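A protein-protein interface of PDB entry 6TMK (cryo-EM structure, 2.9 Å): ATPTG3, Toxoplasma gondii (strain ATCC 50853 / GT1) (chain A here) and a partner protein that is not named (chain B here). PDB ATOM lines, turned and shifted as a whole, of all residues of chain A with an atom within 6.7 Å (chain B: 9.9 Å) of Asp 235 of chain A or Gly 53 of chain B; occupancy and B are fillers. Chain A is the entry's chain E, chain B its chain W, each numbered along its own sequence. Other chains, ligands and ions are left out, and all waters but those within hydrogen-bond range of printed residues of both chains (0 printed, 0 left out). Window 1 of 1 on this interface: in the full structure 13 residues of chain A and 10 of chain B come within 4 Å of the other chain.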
ATOM      1  N   LYS A 197       8.263  -8.657 -16.818  1.00  0.00           N
ATOM      2  CA  LYS A 197       8.625 -10.035 -17.123  1.00  0.00           C
ATOM      3  C   LYS A 197       9.105 -10.176 -18.561  1.00  0.00           C
ATOM      4  O   LYS A 197      10.055 -10.918 -18.830  1.00  0.00           O
ATOM      5  CB  LYS A 197       7.438 -10.953 -16.846  1.00  0.00           C
ATOM      6  CG  LYS A 197       7.631 -12.370 -17.311  1.00  0.00           C
ATOM      7  CD  LYS A 197       6.818 -13.334 -16.492  1.00  0.00           C
ATOM      8  CE  LYS A 197       6.693 -14.667 -17.193  1.00  0.00           C
ATOM      9  NZ  LYS A 197       8.013 -15.313 -17.359  1.00  0.00           N
ATOM     10  N   ILE A 198       8.478  -9.463 -19.495  1.00  0.00           N
ATOM     11  CA  ILE A 198       8.876  -9.571 -20.894  1.00  0.00           C
ATOM     12  C   ILE A 198      10.276  -9.002 -21.086  1.00  0.00           C
ATOM     13  O   ILE A 198      11.135  -9.607 -21.742  1.00  0.00           O
ATOM     14  CB  ILE A 198       7.858  -8.846 -21.792  1.00  0.00           C
ATOM     15  CG1 ILE A 198       6.421  -9.254 -21.456  1.00  0.00           C
ATOM     16  CG2 ILE A 198       8.151  -9.117 -23.250  1.00  0.00           C
ATOM     17  CD1 ILE A 198       6.152 -10.724 -21.490  1.00  0.00           C
ATOM     18  N   ASP A 201      12.821 -11.315 -19.626  1.00  0.00           N
ATOM     19  CA  ASP A 201      13.068 -12.463 -20.487  1.00  0.00           C
ATOM     20  C   ASP A 201      13.992 -12.088 -21.637  1.00  0.00           C
ATOM     21  O   ASP A 201      14.940 -12.818 -21.954  1.00  0.00           O
ATOM     22  CB  ASP A 201      11.745 -13.003 -21.017  1.00  0.00           C
ATOM     23  CG  ASP A 201      10.907 -13.663 -19.939  1.00  0.00           C
ATOM     24  OD1 ASP A 201       9.664 -13.581 -20.019  1.00  0.00           O
ATOM     25  OD2 ASP A 201      11.489 -14.264 -19.013  1.00  0.00           O
ATOM     26  N   PRO A 212      15.601 -21.358 -16.624  1.00  0.00           N
ATOM     27  CA  PRO A 212      14.896 -22.369 -15.838  1.00  0.00           C
ATOM     28  C   PRO A 212      14.866 -23.709 -16.556  1.00  0.00           C
ATOM     29  O   PRO A 212      15.061 -23.810 -17.767  1.00  0.00           O
ATOM     30  CB  PRO A 212      13.489 -21.787 -15.689  1.00  0.00           C
ATOM     31  CG  PRO A 212      13.345 -20.856 -16.819  1.00  0.00           C
ATOM     32  CD  PRO A 212      14.696 -20.294 -17.082  1.00  0.00           C
ATOM     33  N   THR A 214      12.329 -25.467 -17.054  1.00  0.00           N
ATOM     34  CA  THR A 214      11.126 -25.608 -17.857  1.00  0.00           C
ATOM     35  C   THR A 214      11.395 -25.475 -19.347  1.00  0.00           C
ATOM     36  O   THR A 214      10.516 -25.805 -20.147  1.00  0.00           O
ATOM     37  CB  THR A 214      10.091 -24.576 -17.427  1.00  0.00           C
ATOM     38  OG1 THR A 214      10.614 -23.256 -17.618  1.00  0.00           O
ATOM     39  CG2 THR A 214       9.751 -24.766 -15.981  1.00  0.00           C
ATOM     40  N   TYR A 230       3.851 -27.934 -24.013  1.00  0.00           N
ATOM     41  CA  TYR A 230       3.901 -26.483 -23.975  1.00  0.00           C
ATOM     42  C   TYR A 230       2.703 -25.898 -24.704  1.00  0.00           C
ATOM     43  O   TYR A 230       2.297 -26.398 -25.756  1.00  0.00           O
ATOM     44  CB  TYR A 230       5.187 -25.957 -24.610  1.00  0.00           C
ATOM     45  CG  TYR A 230       6.456 -26.372 -23.919  1.00  0.00           C
ATOM     46  CD1 TYR A 230       6.938 -25.664 -22.838  1.00  0.00           C
ATOM     47  CD2 TYR A 230       7.188 -27.454 -24.365  1.00  0.00           C
ATOM     48  CE1 TYR A 230       8.098 -26.031 -22.212  1.00  0.00           C
ATOM     49  CE2 TYR A 230       8.350 -27.827 -23.745  1.00  0.00           C
ATOM     50  CZ  TYR A 230       8.802 -27.111 -22.671  1.00  0.00           C
ATOM     51  OH  TYR A 230       9.961 -27.474 -22.041  1.00  0.00           O
ATOM     52  N   GLY A 232       2.209 -22.952 -26.492  1.00  0.00           N
ATOM     53  CA  GLY A 232       2.655 -21.808 -27.257  1.00  0.00           C
ATOM     54  C   GLY A 232       3.793 -21.022 -26.656  1.00  0.00           C
ATOM     55  O   GLY A 232       4.189 -20.004 -27.233  1.00  0.00           O
ATOM     56  N   ASP A 233       4.342 -21.454 -25.526  1.00  0.00           N
ATOM     57  CA  ASP A 233       5.372 -20.691 -24.844  1.00  0.00           C
ATOM     58  C   ASP A 233       6.011 -21.584 -23.799  1.00  0.00           C
ATOM     59  O   ASP A 233       5.361 -22.471 -23.240  1.00  0.00           O
ATOM     60  CB  ASP A 233       4.794 -19.430 -24.194  1.00  0.00           C
ATOM     61  CG  ASP A 233       5.857 -18.433 -23.806  1.00  0.00           C
ATOM     62  OD1 ASP A 233       6.425 -17.786 -24.708  1.00  0.00           O
ATOM     63  OD2 ASP A 233       6.120 -18.290 -22.597  1.00  0.00           O
ATOM     64  N   ALA A 234       7.296 -21.343 -23.547  1.00  0.00           N
ATOM     65  CA  ALA A 234       8.027 -22.117 -22.556  1.00  0.00           C
ATOM     66  C   ALA A 234       7.577 -21.807 -21.138  1.00  0.00           C
ATOM     67  O   ALA A 234       7.825 -22.609 -20.232  1.00  0.00           O
ATOM     68  CB  ALA A 234       9.522 -21.859 -22.700  1.00  0.00           C
ATOM     69  N   ASP A 235       6.925 -20.669 -20.928  1.00  0.00           N
ATOM     70  CA  ASP A 235       6.421 -20.321 -19.609  1.00  0.00           C
ATOM     71  C   ASP A 235       5.169 -21.100 -19.231  1.00  0.00           C
ATOM     72  O   ASP A 235       4.853 -21.190 -18.042  1.00  0.00           O
ATOM     73  CB  ASP A 235       6.146 -18.819 -19.537  1.00  0.00           C
ATOM     74  CG  ASP A 235       7.372 -17.987 -19.857  1.00  0.00           C
ATOM     75  OD1 ASP A 235       7.273 -17.085 -20.714  1.00  0.00           O
ATOM     76  OD2 ASP A 235       8.438 -18.242 -19.257  1.00  0.00           O
ATOM     77  N   ILE A 236       4.456 -21.665 -20.201  1.00  0.00           N
ATOM     78  CA  ILE A 236       3.183 -22.331 -19.961  1.00  0.00           C
ATOM     79  C   ILE A 236       3.353 -23.778 -20.394  1.00  0.00           C
ATOM     80  O   ILE A 236       3.353 -24.086 -21.592  1.00  0.00           O
ATOM     81  CB  ILE A 236       2.025 -21.662 -20.705  1.00  0.00           C
ATOM     82  CG1 ILE A 236       1.958 -20.175 -20.379  1.00  0.00           C
ATOM     83  CG2 ILE A 236       0.717 -22.320 -20.330  1.00  0.00           C
ATOM     84  CD1 ILE A 236       1.251 -19.378 -21.423  1.00  0.00           C
ATOM     85  N   SER A 237       3.487 -24.674 -19.422  1.00  0.00           N
ATOM     86  CA  SER A 237       3.709 -26.083 -19.687  1.00  0.00           C
ATOM     87  C   SER A 237       2.995 -26.920 -18.638  1.00  0.00           C
ATOM     88  O   SER A 237       2.663 -26.445 -17.550  1.00  0.00           O
ATOM     89  CB  SER A 237       5.200 -26.418 -19.689  1.00  0.00           C
ATOM     90  OG  SER A 237       5.777 -26.155 -18.426  1.00  0.00           O
ATOM     91  N   VAL B  46      -4.706 -27.466  -6.505  1.00  0.00           N
ATOM     92  CA  VAL B  46      -4.974 -26.337  -7.387  1.00  0.00           C
ATOM     93  C   VAL B  46      -4.357 -26.569  -8.757  1.00  0.00           C
ATOM     94  O   VAL B  46      -5.045 -26.540  -9.783  1.00  0.00           O
ATOM     95  CB  VAL B  46      -4.463 -25.033  -6.749  1.00  0.00           C
ATOM     96  CG1 VAL B  46      -4.426 -23.921  -7.754  1.00  0.00           C
ATOM     97  CG2 VAL B  46      -5.339 -24.654  -5.595  1.00  0.00           C
ATOM     98  N   PHE B  47      -3.045 -26.798  -8.795  1.00  0.00           N
ATOM     99  CA  PHE B  47      -2.305 -26.882 -10.045  1.00  0.00           C
ATOM    100  C   PHE B  47      -2.202 -28.308 -10.563  1.00  0.00           C
ATOM    101  O   PHE B  47      -1.233 -28.646 -11.253  1.00  0.00           O
ATOM    102  CB  PHE B  47      -0.917 -26.274  -9.863  1.00  0.00           C
ATOM    103  CG  PHE B  47      -0.938 -24.798  -9.643  1.00  0.00           C
ATOM    104  CD1 PHE B  47      -0.695 -24.280  -8.393  1.00  0.00           C
ATOM    105  CD2 PHE B  47      -1.229 -23.931 -10.676  1.00  0.00           C
ATOM    106  CE1 PHE B  47      -0.725 -22.928  -8.176  1.00  0.00           C
ATOM    107  CE2 PHE B  47      -1.258 -22.577 -10.466  1.00  0.00           C
ATOM    108  CZ  PHE B  47      -1.009 -22.073  -9.213  1.00  0.00           C
ATOM    109  N   GLN B  49      -4.483 -29.919 -12.798  1.00  0.00           N
ATOM    110  CA  GLN B  49      -4.757 -29.881 -14.226  1.00  0.00           C
ATOM    111  C   GLN B  49      -4.320 -28.570 -14.864  1.00  0.00           C
ATOM    112  O   GLN B  49      -3.733 -28.578 -15.951  1.00  0.00           O
ATOM    113  CB  GLN B  49      -6.248 -30.112 -14.480  1.00  0.00           C
ATOM    114  CG  GLN B  49      -6.630 -30.194 -15.953  1.00  0.00           C
ATOM    115  CD  GLN B  49      -5.867 -31.271 -16.700  1.00  0.00           C
ATOM    116  OE1 GLN B  49      -6.360 -32.385 -16.880  1.00  0.00           O
ATOM    117  NE2 GLN B  49      -4.657 -30.944 -17.142  1.00  0.00           N
ATOM    118  N   ILE B  50      -4.591 -27.442 -14.218  1.00  0.00           N
ATOM    119  CA  ILE B  50      -4.172 -26.150 -14.750  1.00  0.00           C
ATOM    120  C   ILE B  50      -2.659 -26.052 -14.628  1.00  0.00           C
ATOM    121  O   ILE B  50      -2.064 -26.707 -13.760  1.00  0.00           O
ATOM    122  CB  ILE B  50      -4.850 -24.980 -14.023  1.00  0.00           C
ATOM    123  CG1 ILE B  50      -4.493 -24.982 -12.542  1.00  0.00           C
ATOM    124  CG2 ILE B  50      -6.348 -25.081 -14.162  1.00  0.00           C
ATOM    125  CD1 ILE B  50      -4.856 -23.710 -11.844  1.00  0.00           C
ATOM    126  N   PRO B  51      -1.998 -25.247 -15.448  1.00  0.00           N
ATOM    127  CA  PRO B  51      -0.548 -25.120 -15.344  1.00  0.00           C
ATOM    128  C   PRO B  51      -0.135 -24.126 -14.269  1.00  0.00           C
ATOM    129  O   PRO B  51      -0.919 -23.302 -13.796  1.00  0.00           O
ATOM    130  CB  PRO B  51      -0.155 -24.630 -16.737  1.00  0.00           C
ATOM    131  CG  PRO B  51      -1.284 -23.788 -17.125  1.00  0.00           C
ATOM    132  CD  PRO B  51      -2.513 -24.483 -16.596  1.00  0.00           C
ATOM    133  N   ASP B  52       1.139 -24.224 -13.895  1.00  0.00           N
ATOM    134  CA  ASP B  52       1.775 -23.337 -12.930  1.00  0.00           C
ATOM    135  C   ASP B  52       2.423 -22.131 -13.588  1.00  0.00           C
ATOM    136  O   ASP B  52       3.375 -21.565 -13.039  1.00  0.00           O
ATOM    137  CB  ASP B  52       2.811 -24.112 -12.120  1.00  0.00           C
ATOM    138  CG  ASP B  52       4.021 -24.495 -12.945  1.00  0.00           C
ATOM    139  OD1 ASP B  52       3.915 -25.448 -13.748  1.00  0.00           O
ATOM    140  OD2 ASP B  52       5.075 -23.844 -12.793  1.00  0.00           O
ATOM    141  N   GLY B  53       1.933 -21.724 -14.754  1.00  0.00           N
ATOM    142  CA  GLY B  53       2.533 -20.603 -15.448  1.00  0.00           C
ATOM    143  C   GLY B  53       2.224 -19.291 -14.758  1.00  0.00           C
ATOM    144  O   GLY B  53       1.111 -19.051 -14.290  1.00  0.00           O
ATOM    145  N   LEU B  54       3.235 -18.430 -14.704  1.00  0.00           N
ATOM    146  CA  LEU B  54       3.121 -17.145 -14.029  1.00  0.00           C
ATOM    147  C   LEU B  54       2.711 -17.331 -12.573  1.00  0.00           C
ATOM    148  O   LEU B  54       1.891 -16.585 -12.037  1.00  0.00           O
ATOM    149  CB  LEU B  54       2.126 -16.238 -14.756  1.00  0.00           C
ATOM    150  CG  LEU B  54       2.542 -15.578 -16.067  1.00  0.00           C
ATOM    151  CD1 LEU B  54       3.100 -16.576 -17.071  1.00  0.00           C
ATOM    152  CD2 LEU B  54       1.334 -14.855 -16.634  1.00  0.00           C
ATOM    153  N   LEU B  55       3.280 -18.345 -11.925  1.00  0.00           N
ATOM    154  CA  LEU B  55       2.922 -18.622 -10.542  1.00  0.00           C
ATOM    155  C   LEU B  55       3.551 -17.608  -9.599  1.00  0.00           C
ATOM    156  O   LEU B  55       2.859 -17.001  -8.776  1.00  0.00           O
ATOM    157  CB  LEU B  55       3.346 -20.040 -10.177  1.00  0.00           C
ATOM    158  CG  LEU B  55       3.225 -20.474  -8.716  1.00  0.00           C
ATOM    159  CD1 LEU B  55       1.915 -20.056  -8.105  1.00  0.00           C
ATOM    160  CD2 LEU B  55       3.393 -21.968  -8.613  1.00  0.00           C
ATOM    161  N   GLY B  56       4.857 -17.395  -9.714  1.00  0.00           N
ATOM    162  CA  GLY B  56       5.563 -16.498  -8.829  1.00  0.00           C
ATOM    163  C   GLY B  56       5.756 -15.092  -9.351  1.00  0.00           C
ATOM    164  O   GLY B  56       6.534 -14.334  -8.761  1.00  0.00           O
ATOM    165  N   HIS B  57       5.076 -14.713 -10.432  1.00  0.00           N
ATOM    166  CA  HIS B  57       5.269 -13.415 -11.062  1.00  0.00           C
ATOM    167  C   HIS B  57       4.018 -12.553 -11.010  1.00  0.00           C
ATOM    168  O   HIS B  57       3.982 -11.493 -11.644  1.00  0.00           O
ATOM    169  CB  HIS B  57       5.712 -13.594 -12.513  1.00  0.00           C
ATOM    170  CG  HIS B  57       6.970 -14.388 -12.667  1.00  0.00           C
ATOM    171  ND1 HIS B  57       8.220 -13.847 -12.464  1.00  0.00           N
ATOM    172  CD2 HIS B  57       7.170 -15.683 -13.007  1.00  0.00           C
ATOM    173  CE1 HIS B  57       9.137 -14.775 -12.672  1.00  0.00           C
ATOM    174  NE2 HIS B  57       8.525 -15.897 -13.003  1.00  0.00           N
ATOM    175  N   THR B  58       2.997 -12.970 -10.270  1.00  0.00           N
ATOM    176  CA  THR B  58       1.744 -12.236 -10.222  1.00  0.00           C
ATOM    177  C   THR B  58       1.716 -11.215  -9.095  1.00  0.00           C
ATOM    178  O   THR B  58       0.979 -10.227  -9.184  1.00  0.00           O
ATOM    179  CB  THR B  58       0.580 -13.219 -10.085  1.00  0.00           C
ATOM    180  OG1 THR B  58       0.807 -14.096  -8.979  1.00  0.00           O
ATOM    181  CG2 THR B  58       0.440 -14.034 -11.345  1.00  0.00           C
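Gly 53 of chain B touches just one residue of chain A: Asp 235 (3.5 Å).
No residue of chain B comes within 4 Å of Asp 233 of chain A.
No residue of chain B comes within 4 Å of Ile 236 of chain A.
Of the printed residues of chain A, His 57 of chain B touches Lys 197.
Printed residues of chain B within 4 Å of Lys 197 of chain A: His 57.
Printed residues of chain B within 4 Å of Ser 237 of chain A: Pro 51 (3.4 Å).
Printed residues of chain A within 4 Å of Pro 51 of chain B: Ser 237.
Leu 55 of chain B touches none of the printed residues of chain A.
Thr 214 of chain A touches none of the printed residues of chain B.
The nearest residue of chain B that does not touch Asp 235 of chain A is Leu 54 of chain B (4.5 Å).
The nearest residue of chain A that does not touch Gly 53 of chain B is Ile 236 of chain A (4.9 Å).
The nearest printed residue of chain A that does not touch His 57 of chain B is Asp 235 of chain A (6.7 Å).
His 57 of chain B touches Lys 197 of chain A.
Asp 235 of chain A touches Gly 53 of chain B.
Pro 51 of chain B touches Ser 237 of chain A (CB to O, 3.4 Å).
The side-chain carboxylate (OD2) of Asp 235 of chain A is in salt-bridge range of the side-chain amino group (NZ) of Lys 197 of chain A (3.5 Å).
OD2 of Asp 233 of chain A lies within hydrogen-bond range of N of Asp 235 of chain A (3.0 Å).
NZ of Lys 197 of chain A is in salt-bridge range of OD1 of Asp 201 of chain A (3.6 Å).
Along chain B the printed residues that touch a printed residue of chain A span positions 51 to 57.
Among the printed residues, no Asp or Glu carboxylate lies within 4 Å of a Lys or Arg side-chain nitrogen of the other chain.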
